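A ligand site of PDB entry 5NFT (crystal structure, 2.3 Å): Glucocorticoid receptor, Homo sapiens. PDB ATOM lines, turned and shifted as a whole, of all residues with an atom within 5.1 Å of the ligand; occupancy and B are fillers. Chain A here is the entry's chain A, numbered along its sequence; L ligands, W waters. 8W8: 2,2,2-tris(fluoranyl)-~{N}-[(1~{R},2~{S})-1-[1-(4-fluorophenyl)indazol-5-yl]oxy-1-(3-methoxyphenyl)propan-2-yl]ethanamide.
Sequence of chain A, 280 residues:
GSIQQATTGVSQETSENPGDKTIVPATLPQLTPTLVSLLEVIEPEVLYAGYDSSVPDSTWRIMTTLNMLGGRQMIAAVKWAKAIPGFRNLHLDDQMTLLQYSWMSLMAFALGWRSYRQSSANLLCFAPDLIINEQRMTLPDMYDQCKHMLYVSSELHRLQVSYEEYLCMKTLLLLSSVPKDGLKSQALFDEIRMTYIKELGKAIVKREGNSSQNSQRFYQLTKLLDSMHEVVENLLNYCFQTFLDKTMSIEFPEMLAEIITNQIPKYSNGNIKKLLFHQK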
ATOM      1  N   ILE A  62      -8.091  18.646  -0.862  1.00  0.00           N
ATOM      2  CA  ILE A  62      -7.158  19.588  -0.246  1.00  0.00           C
ATOM      3  C   ILE A  62      -6.216  18.868   0.736  1.00  0.00           C
ATOM      4  O   ILE A  62      -5.003  19.046   0.629  1.00  0.00           O
ATOM      5  CB  ILE A  62      -7.903  20.795   0.367  1.00  0.00           C
ATOM      6  CG1 ILE A  62      -8.574  21.641  -0.755  1.00  0.00           C
ATOM      7  CG2 ILE A  62      -6.960  21.642   1.225  1.00  0.00           C
ATOM      8  CD1 ILE A  62      -9.651  22.624  -0.312  1.00  0.00           C
ATOM      9  N   MET A  63      -6.760  18.013   1.622  1.00  0.00           N
ATOM     10  CA  MET A  63      -5.995  17.216   2.585  1.00  0.00           C
ATOM     11  C   MET A  63      -4.936  16.349   1.875  1.00  0.00           C
ATOM     12  O   MET A  63      -3.796  16.302   2.322  1.00  0.00           O
ATOM     13  CB  MET A  63      -6.942  16.351   3.424  1.00  0.00           C
ATOM     14  CG  MET A  63      -6.264  15.662   4.594  1.00  0.00           C
ATOM     15  SD  MET A  63      -7.418  15.040   5.839  1.00  0.00           S
ATOM     16  CE  MET A  63      -8.278  16.561   6.315  1.00  0.00           C
ATOM     17  N   LEU A  66      -2.257  18.656   0.350  1.00  0.00           N
ATOM     18  CA  LEU A  66      -1.441  19.199   1.430  1.00  0.00           C
ATOM     19  C   LEU A  66      -0.505  18.180   2.041  1.00  0.00           C
ATOM     20  O   LEU A  66       0.603  18.548   2.440  1.00  0.00           O
ATOM     21  CB  LEU A  66      -2.293  19.897   2.504  1.00  0.00           C
ATOM     22  CG  LEU A  66      -2.992  21.184   2.052  1.00  0.00           C
ATOM     23  CD1 LEU A  66      -3.762  21.810   3.200  1.00  0.00           C
ATOM     24  CD2 LEU A  66      -1.994  22.178   1.470  1.00  0.00           C
ATOM     25  N   ASN A  67      -0.895  16.888   2.058  1.00  0.00           N
ATOM     26  CA  ASN A  67      -0.023  15.816   2.542  1.00  0.00           C
ATOM     27  C   ASN A  67       1.134  15.653   1.582  1.00  0.00           C
ATOM     28  O   ASN A  67       2.263  15.572   2.036  1.00  0.00           O
ATOM     29  CB  ASN A  67      -0.775  14.492   2.691  1.00  0.00           C
ATOM     30  CG  ASN A  67      -1.627  14.442   3.912  1.00  0.00           C
ATOM     31  OD1 ASN A  67      -1.524  15.282   4.804  1.00  0.00           O
ATOM     32  ND2 ASN A  67      -2.495  13.443   3.988  1.00  0.00           N
ATOM     33  N   LEU A  69       2.300  17.932  -0.572  1.00  0.00           N
ATOM     34  CA  LEU A  69       3.102  19.146  -0.420  1.00  0.00           C
ATOM     35  C   LEU A  69       3.950  19.062   0.856  1.00  0.00           C
ATOM     36  O   LEU A  69       5.124  19.421   0.825  1.00  0.00           O
ATOM     37  CB  LEU A  69       2.190  20.397  -0.408  1.00  0.00           C
ATOM     38  CG  LEU A  69       2.850  21.788  -0.164  1.00  0.00           C
ATOM     39  CD1 LEU A  69       3.970  22.068  -1.212  1.00  0.00           C
ATOM     40  CD2 LEU A  69       1.790  22.906  -0.159  1.00  0.00           C
ATOM     41  N   GLY A  70       3.343  18.575   1.951  1.00  0.00           N
ATOM     42  CA  GLY A  70       3.985  18.395   3.238  1.00  0.00           C
ATOM     43  C   GLY A  70       5.233  17.534   3.196  1.00  0.00           C
ATOM     44  O   GLY A  70       6.207  17.824   3.894  1.00  0.00           O
ATOM     45  N   GLN A  73       7.898  19.707   1.735  1.00  0.00           N
ATOM     46  CA  GLN A  73       8.291  20.703   2.751  1.00  0.00           C
ATOM     47  C   GLN A  73       9.286  20.063   3.717  1.00  0.00           C
ATOM     48  O   GLN A  73      10.262  20.693   4.100  1.00  0.00           O
ATOM     49  CB  GLN A  73       7.057  21.195   3.570  1.00  0.00           C
ATOM     50  CG  GLN A  73       5.932  21.831   2.745  1.00  0.00           C
ATOM     51  CD  GLN A  73       6.183  23.221   2.214  1.00  0.00           C
ATOM     52  OE1 GLN A  73       7.319  23.709   2.092  1.00  0.00           O
ATOM     53  NE2 GLN A  73       5.103  23.895   1.848  1.00  0.00           N
ATOM     54  N   TRP A 103       9.143  17.631  13.321  1.00  0.00           N
ATOM     55  CA  TRP A 103       8.562  17.846  11.984  1.00  0.00           C
ATOM     56  C   TRP A 103       7.258  18.711  11.972  1.00  0.00           C
ATOM     57  O   TRP A 103       7.217  19.732  11.290  1.00  0.00           O
ATOM     58  CB  TRP A 103       8.349  16.503  11.258  1.00  0.00           C
ATOM     59  CG  TRP A 103       7.184  15.692  11.729  1.00  0.00           C
ATOM     60  CD1 TRP A 103       7.085  15.022  12.913  1.00  0.00           C
ATOM     61  CD2 TRP A 103       5.950  15.479  11.040  1.00  0.00           C
ATOM     62  NE1 TRP A 103       5.863  14.410  13.005  1.00  0.00           N
ATOM     63  CE2 TRP A 103       5.154  14.656  11.858  1.00  0.00           C
ATOM     64  CE3 TRP A 103       5.432  15.923   9.809  1.00  0.00           C
ATOM     65  CZ2 TRP A 103       3.872  14.224  11.478  1.00  0.00           C
ATOM     66  CZ3 TRP A 103       4.156  15.506   9.444  1.00  0.00           C
ATOM     67  CH2 TRP A 103       3.394  14.669  10.262  1.00  0.00           C
ATOM     68  N   MET A 104       6.229  18.329  12.752  1.00  0.00           N
ATOM     69  CA  MET A 104       4.955  19.055  12.778  1.00  0.00           C
ATOM     70  C   MET A 104       5.075  20.429  13.429  1.00  0.00           C
ATOM     71  O   MET A 104       4.396  21.369  13.008  1.00  0.00           O
ATOM     72  CB  MET A 104       3.832  18.200  13.418  1.00  0.00           C
ATOM     73  CG  MET A 104       2.435  18.854  13.322  1.00  0.00           C
ATOM     74  SD  MET A 104       1.971  19.329  11.625  1.00  0.00           S
ATOM     75  CE  MET A 104       1.267  17.775  11.065  1.00  0.00           C
ATOM     76  N   MET A 107       6.612  22.627  10.745  1.00  0.00           N
ATOM     77  CA  MET A 107       5.620  22.884   9.713  1.00  0.00           C
ATOM     78  C   MET A 107       4.518  23.828  10.153  1.00  0.00           C
ATOM     79  O   MET A 107       4.218  24.774   9.430  1.00  0.00           O
ATOM     80  CB  MET A 107       5.081  21.568   9.160  1.00  0.00           C
ATOM     81  CG  MET A 107       6.153  20.843   8.357  1.00  0.00           C
ATOM     82  SD  MET A 107       5.575  20.109   6.842  1.00  0.00           S
ATOM     83  CE  MET A 107       4.566  18.769   7.521  1.00  0.00           C
ATOM     84  N   ALA A 108       3.963  23.628  11.364  1.00  0.00           N
ATOM     85  CA  ALA A 108       2.930  24.520  11.922  1.00  0.00           C
ATOM     86  C   ALA A 108       3.479  25.947  12.122  1.00  0.00           C
ATOM     87  O   ALA A 108       2.800  26.915  11.765  1.00  0.00           O
ATOM     88  CB  ALA A 108       2.404  23.952  13.235  1.00  0.00           C
ATOM     89  N   ALA A 110       6.311  27.417  10.636  1.00  0.00           N
ATOM     90  CA  ALA A 110       6.664  28.013   9.347  1.00  0.00           C
ATOM     91  C   ALA A 110       5.385  28.456   8.608  1.00  0.00           C
ATOM     92  O   ALA A 110       5.352  29.533   8.044  1.00  0.00           O
ATOM     93  CB  ALA A 110       7.496  27.043   8.511  1.00  0.00           C
ATOM     94  N   LEU A 111       4.317  27.624   8.681  1.00  0.00           N
ATOM     95  CA  LEU A 111       3.028  27.949   8.068  1.00  0.00           C
ATOM     96  C   LEU A 111       2.388  29.202   8.723  1.00  0.00           C
ATOM     97  O   LEU A 111       1.899  30.090   8.026  1.00  0.00           O
ATOM     98  CB  LEU A 111       2.070  26.748   8.136  1.00  0.00           C
ATOM     99  CG  LEU A 111       0.612  27.012   7.692  1.00  0.00           C
ATOM    100  CD1 LEU A 111       0.517  27.396   6.202  1.00  0.00           C
ATOM    101  CD2 LEU A 111      -0.270  25.831   8.024  1.00  0.00           C
ATOM    102  N   ARG A 114       4.185  32.323   7.538  1.00  0.00           N
ATOM    103  CA  ARG A 114       3.783  32.649   6.178  1.00  0.00           C
ATOM    104  C   ARG A 114       2.378  33.227   6.091  1.00  0.00           C
ATOM    105  O   ARG A 114       2.155  34.148   5.320  1.00  0.00           O
ATOM    106  CB  ARG A 114       3.969  31.479   5.218  1.00  0.00           C
ATOM    107  CG  ARG A 114       4.446  31.996   3.872  1.00  0.00           C
ATOM    108  CD  ARG A 114       4.756  30.911   2.898  1.00  0.00           C
ATOM    109  NE  ARG A 114       6.049  30.260   3.156  1.00  0.00           N
ATOM    110  CZ  ARG A 114       6.385  29.101   2.612  1.00  0.00           C
ATOM    111  NH1 ARG A 114       7.573  28.574   2.880  1.00  0.00           N
ATOM    112  NH2 ARG A 114       5.562  28.467   1.805  1.00  0.00           N
ATOM    113  N   CYS A 125      -1.873  30.189   4.475  1.00  0.00           N
ATOM    114  CA  CYS A 125      -1.143  30.258   3.219  1.00  0.00           C
ATOM    115  C   CYS A 125      -0.194  29.071   3.057  1.00  0.00           C
ATOM    116  O   CYS A 125       1.025  29.222   3.210  1.00  0.00           O
ATOM    117  CB  CYS A 125      -0.419  31.607   3.075  1.00  0.00           C
ATOM    118  SG  CYS A 125      -1.498  33.052   3.259  1.00  0.00           S
ATOM    119  N   PHE A 126      -0.755  27.899   2.766  1.00  0.00           N
ATOM    120  CA  PHE A 126       0.004  26.658   2.592  1.00  0.00           C
ATOM    121  C   PHE A 126       0.936  26.746   1.392  1.00  0.00           C
ATOM    122  O   PHE A 126       2.070  26.280   1.445  1.00  0.00           O
ATOM    123  CB  PHE A 126      -0.928  25.458   2.453  1.00  0.00           C
ATOM    124  CG  PHE A 126      -1.479  24.900   3.746  1.00  0.00           C
ATOM    125  CD1 PHE A 126      -0.778  23.924   4.458  1.00  0.00           C
ATOM    126  CD2 PHE A 126      -2.718  25.310   4.228  1.00  0.00           C
ATOM    127  CE1 PHE A 126      -1.301  23.382   5.628  1.00  0.00           C
ATOM    128  CE2 PHE A 126      -3.249  24.762   5.400  1.00  0.00           C
ATOM    129  CZ  PHE A 126      -2.529  23.809   6.101  1.00  0.00           C
ATOM    130  N   MET A 142     -12.879  20.594   7.576  1.00  0.00           N
ATOM    131  CA  MET A 142     -11.684  21.398   7.276  1.00  0.00           C
ATOM    132  C   MET A 142     -11.123  22.135   8.485  1.00  0.00           C
ATOM    133  O   MET A 142      -9.912  22.141   8.699  1.00  0.00           O
ATOM    134  CB  MET A 142     -11.948  22.379   6.118  1.00  0.00           C
ATOM    135  CG  MET A 142     -10.688  23.093   5.621  1.00  0.00           C
ATOM    136  SD  MET A 142      -9.442  21.976   4.937  1.00  0.00           S
ATOM    137  CE  MET A 142     -10.052  21.801   3.325  1.00  0.00           C
ATOM    138  N   GLN A 145      -8.684  20.597  11.879  1.00  0.00           N
ATOM    139  CA  GLN A 145      -7.233  20.574  11.786  1.00  0.00           C
ATOM    140  C   GLN A 145      -6.654  21.994  11.562  1.00  0.00           C
ATOM    141  O   GLN A 145      -5.647  22.348  12.180  1.00  0.00           O
ATOM    142  CB  GLN A 145      -6.778  19.563  10.714  1.00  0.00           C
ATOM    143  CG  GLN A 145      -5.345  19.081  10.865  1.00  0.00           C
ATOM    144  CD  GLN A 145      -5.042  18.214  12.077  1.00  0.00           C
ATOM    145  OE1 GLN A 145      -5.587  18.391  13.173  1.00  0.00           O
ATOM    146  NE2 GLN A 145      -4.060  17.337  11.935  1.00  0.00           N
ATOM    147  N   CYS A 146      -7.316  22.800  10.721  1.00  0.00           N
ATOM    148  CA  CYS A 146      -6.917  24.160  10.374  1.00  0.00           C
ATOM    149  C   CYS A 146      -6.917  25.147  11.553  1.00  0.00           C
ATOM    150  O   CYS A 146      -6.129  26.088  11.538  1.00  0.00           O
ATOM    151  CB  CYS A 146      -7.739  24.696   9.209  1.00  0.00           C
ATOM    152  SG  CYS A 146      -7.329  23.934   7.615  1.00  0.00           S
ATOM    153  N   MET A 149      -3.565  25.482  13.378  1.00  0.00           N
ATOM    154  CA  MET A 149      -2.668  26.253  12.531  1.00  0.00           C
ATOM    155  C   MET A 149      -3.028  27.742  12.647  1.00  0.00           C
ATOM    156  O   MET A 149      -2.121  28.586  12.688  1.00  0.00           O
ATOM    157  CB  MET A 149      -2.759  25.791  11.059  1.00  0.00           C
ATOM    158  CG  MET A 149      -2.372  24.345  10.839  1.00  0.00           C
ATOM    159  SD  MET A 149      -0.668  24.061  11.355  1.00  0.00           S
ATOM    160  CE  MET A 149      -0.341  22.478  10.523  1.00  0.00           C
ATOM    161  N   LEU A 235      -2.633  18.424  16.517  1.00  0.00           N
ATOM    162  CA  LEU A 235      -2.426  18.144  15.086  1.00  0.00           C
ATOM    163  C   LEU A 235      -2.070  16.676  14.875  1.00  0.00           C
ATOM    164  O   LEU A 235      -2.604  16.047  13.967  1.00  0.00           O
ATOM    165  CB  LEU A 235      -1.303  19.027  14.510  1.00  0.00           C
ATOM    166  CG  LEU A 235      -1.629  20.519  14.279  1.00  0.00           C
ATOM    167  CD1 LEU A 235      -0.370  21.299  14.058  1.00  0.00           C
ATOM    168  CD2 LEU A 235      -2.591  20.712  13.114  1.00  0.00           C
ATOM    169  N   TYR A 238      -5.052  13.905  15.350  1.00  0.00           N
ATOM    170  CA  TYR A 238      -5.861  13.811  14.136  1.00  0.00           C
ATOM    171  C   TYR A 238      -5.046  13.162  13.006  1.00  0.00           C
ATOM    172  O   TYR A 238      -5.557  12.294  12.309  1.00  0.00           O
ATOM    173  CB  TYR A 238      -6.328  15.220  13.741  1.00  0.00           C
ATOM    174  CG  TYR A 238      -7.292  15.249  12.578  1.00  0.00           C
ATOM    175  CD1 TYR A 238      -6.833  15.235  11.262  1.00  0.00           C
ATOM    176  CD2 TYR A 238      -8.661  15.330  12.785  1.00  0.00           C
ATOM    177  CE1 TYR A 238      -7.718  15.260  10.190  1.00  0.00           C
ATOM    178  CE2 TYR A 238      -9.561  15.362  11.721  1.00  0.00           C
ATOM    179  CZ  TYR A 238      -9.078  15.338  10.424  1.00  0.00           C
ATOM    180  OH  TYR A 238      -9.948  15.379   9.357  1.00  0.00           O
ATOM    181  N   CYS A 239      -3.786  13.619  12.811  1.00  0.00           N
ATOM    182  CA  CYS A 239      -2.891  13.129  11.770  1.00  0.00           C
ATOM    183  C   CYS A 239      -2.591  11.627  11.888  1.00  0.00           C
ATOM    184  O   CYS A 239      -2.628  10.917  10.881  1.00  0.00           O
ATOM    185  CB  CYS A 239      -1.605  13.959  11.720  1.00  0.00           C
ATOM    186  SG  CYS A 239      -0.516  13.565  10.330  1.00  0.00           S
ATOM    187  N   THR A 242      -5.810   9.612  10.990  1.00  0.00           N
ATOM    188  CA  THR A 242      -6.024   9.711   9.538  1.00  0.00           C
ATOM    189  C   THR A 242      -5.066   8.774   8.789  1.00  0.00           C
ATOM    190  O   THR A 242      -5.481   8.111   7.831  1.00  0.00           O
ATOM    191  CB  THR A 242      -5.930  11.186   9.093  1.00  0.00           C
ATOM    192  OG1 THR A 242      -6.794  11.987   9.896  1.00  0.00           O
ATOM    193  CG2 THR A 242      -6.293  11.377   7.641  1.00  0.00           C
ATOM    194  N   ILE A 250      -6.792   8.375   2.635  1.00  0.00           N
ATOM    195  CA  ILE A 250      -5.987   9.595   2.726  1.00  0.00           C
ATOM    196  C   ILE A 250      -4.520   9.213   2.542  1.00  0.00           C
ATOM    197  O   ILE A 250      -3.925   8.546   3.388  1.00  0.00           O
ATOM    198  CB  ILE A 250      -6.283  10.469   3.987  1.00  0.00           C
ATOM    199  CG1 ILE A 250      -7.734  11.045   3.954  1.00  0.00           C
ATOM    200  CG2 ILE A 250      -5.236  11.591   4.172  1.00  0.00           C
ATOM    201  CD1 ILE A 250      -7.968  12.263   3.021  1.00  0.00           C
ATOM    202  N   PHE A 252      -0.478   9.705   2.148  1.00  0.00           N
ATOM    203  CA  PHE A 252       0.658  10.389   2.737  1.00  0.00           C
ATOM    204  C   PHE A 252       1.865   9.988   1.910  1.00  0.00           C
ATOM    205  O   PHE A 252       2.013   8.798   1.585  1.00  0.00           O
ATOM    206  CB  PHE A 252       0.855   9.971   4.199  1.00  0.00           C
ATOM    207  CG  PHE A 252      -0.148  10.569   5.165  1.00  0.00           C
ATOM    208  CD1 PHE A 252      -1.405  10.000   5.322  1.00  0.00           C
ATOM    209  CD2 PHE A 252       0.184  11.669   5.952  1.00  0.00           C
ATOM    210  CE1 PHE A 252      -2.329  10.541   6.213  1.00  0.00           C
ATOM    211  CE2 PHE A 252      -0.729  12.202   6.860  1.00  0.00           C
ATOM    212  CZ  PHE A 252      -1.977  11.628   6.997  1.00  0.00           C
ATOM    213  N   LEU A 256       6.431  11.580   4.810  1.00  0.00           N
ATOM    214  CA  LEU A 256       5.534  11.697   5.963  1.00  0.00           C
ATOM    215  C   LEU A 256       5.171  10.351   6.549  1.00  0.00           C
ATOM    216  O   LEU A 256       5.180  10.222   7.778  1.00  0.00           O
ATOM    217  CB  LEU A 256       4.277  12.544   5.641  1.00  0.00           C
ATOM    218  CG  LEU A 256       4.538  14.002   5.177  1.00  0.00           C
ATOM    219  CD1 LEU A 256       3.251  14.798   5.149  1.00  0.00           C
ATOM    220  CD2 LEU A 256       5.586  14.704   6.060  1.00  0.00           C
HETATM  221  C1  8W8 L   1      -3.297  20.623   8.291  1.00  0.00           C
HETATM  222  C2  8W8 L   1      -2.130  19.898   8.160  1.00  0.00           C
HETATM  223  C3  8W8 L   1       2.154  22.102   6.930  1.00  0.00           C
HETATM  224  C7  8W8 L   1       1.508  21.029   7.514  1.00  0.00           C
HETATM  225  C8  8W8 L   1       5.169  25.338   5.977  1.00  0.00           C
HETATM  226  C9  8W8 L   1       3.842  26.437   4.291  1.00  0.00           C
HETATM  227  C10 8W8 L   1       1.003  19.983   5.398  1.00  0.00           C
HETATM  228  C11 8W8 L   1      -2.990  18.836   6.192  1.00  0.00           C
HETATM  229  C12 8W8 L   1       1.884  21.413   3.456  1.00  0.00           C
HETATM  230  C13 8W8 L   1       1.631  21.059   4.799  1.00  0.00           C
HETATM  231  C14 8W8 L   1      -1.955  19.001   7.110  1.00  0.00           C
HETATM  232  C15 8W8 L   1       2.191  22.081   5.551  1.00  0.00           C
HETATM  233  C16 8W8 L   1       3.448  24.140   4.872  1.00  0.00           C
HETATM  234  C19 8W8 L   1       4.859  26.455   5.234  1.00  0.00           C
HETATM  235  C20 8W8 L   1      -2.857  15.939   8.399  1.00  0.00           C
HETATM  236  C21 8W8 L   1       0.558  16.095   7.543  1.00  0.00           C
HETATM  237  C22 8W8 L   1      -6.348  20.056   5.645  1.00  0.00           C
HETATM  238  C24 8W8 L   1      -0.710  16.920   7.733  1.00  0.00           C
HETATM  239  N26 8W8 L   1       2.560  22.557   3.357  1.00  0.00           N
HETATM  240  C4  8W8 L   1       4.467  24.170   5.808  1.00  0.00           C
HETATM  241  C5  8W8 L   1       3.147  25.258   4.118  1.00  0.00           C
HETATM  242  C6  8W8 L   1      -4.327  20.452   7.378  1.00  0.00           C
HETATM  243  C17 8W8 L   1       0.945  20.000   6.778  1.00  0.00           C
HETATM  244  C18 8W8 L   1      -4.169  19.548   6.341  1.00  0.00           C
HETATM  245  C23 8W8 L   1      -0.673  18.224   6.952  1.00  0.00           C
HETATM  246  C25 8W8 L   1      -4.092  15.228   7.920  1.00  0.00           C
HETATM  247  N27 8W8 L   1       2.741  22.950   4.634  1.00  0.00           N
HETATM  248  N28 8W8 L   1      -1.872  16.091   7.446  1.00  0.00           N
HETATM  249  O29 8W8 L   1      -2.809  16.331   9.559  1.00  0.00           O
HETATM  250  O30 8W8 L   1      -5.154  19.308   5.379  1.00  0.00           O
HETATM  251  O31 8W8 L   1       0.383  18.972   7.541  1.00  0.00           O
HETATM  252  F32 8W8 L   1       5.560  27.580   5.428  1.00  0.00           F
HETATM  253  F33 8W8 L   1      -5.138  16.099   7.826  1.00  0.00           F
HETATM  254  F34 8W8 L   1      -4.500  14.303   8.814  1.00  0.00           F
HETATM  255  F35 8W8 L   1      -3.948  14.592   6.725  1.00  0.00           F
HETATM  256  O   HOH W   1       8.117  23.925   6.502  1.00  0.00           O
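OD1 of Asn 67 lies within hydrogen-bond range of N28 of the ligand (2.8 Å). NE2 of Gln 145 sits at hydrogen-bond distance from O29 of the ligand, at 2.9 Å. The side-chain amide nitrogen (NE2) of Gln 73 sits at hydrogen-bond distance from a nitrogen (N26) of the ligand. SG of Cys 239 sits close to O29 of the ligand, at 3.7 Å.
The side-chain amide nitrogen (NE2) of Gln 145 lies within hydrogen-bond range of the backbone carbonyl oxygen (O) of Leu 235, at 2.8 Å. The backbone carbonyl oxygen (O) of Tyr 238 is in hydrogen-bond range of the side-chain hydroxyl (OG1) of Thr 242 (2.7 Å). The backbone carbonyl oxygen of Met 142 is in hydrogen-bond range of the side-chain sulfur of Cys 146, 3.3 Å away.
The side-chain sulfur (SD) of Met 63 lies close to a fluorine (F33) of the ligand (3.2 Å). The backbone carbonyl oxygen (O) of Ala 110 lies close to a fluorine (F32) of the ligand (3.3 Å). A fluorine (F32) of the ligand sits close to the backbone NH of Leu 111. The guanidinium group (NH1) of Arg 114 lies close to a fluorine (F32) of the ligand. The side-chain hydroxyl (OG1) of Thr 242 sits close to a fluorine (F34) of the ligand (3.4 Å). Merely in contact with the ligand: Leu 66 (3.3 Å), Leu 69 (3.6 Å), Gly 70 (3.5 Å), Met 104 (3.8 Å), Met 107 (3.6 Å), Phe 126 (3.1 Å), Met 142 (3.7 Å), Met 149 (3.8 Å), Tyr 238 (3.5 Å), Phe 252 (3.6 Å) and Leu 256 (3.8 Å). Hydrophobic or aromatic side chains that line the ligand: Met 63, Leu 66, Leu 69, Met 104, Met 107, Ala 110, Leu 111, Phe 126, Met 142, Met 149, Tyr 238, Phe 252 and Leu 256. 20 residues have an atom within 4 Å of the ligand: Met 63, Leu 66, Asn 67, Leu 69, Gly 70, Gln 73, Met 104, Met 107, Ala 110, Leu 111, Arg 114, Phe 126, Met 142, Gln 145, Met 149, Tyr 238, Cys 239, Thr 242, Phe 252 and Leu 256.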
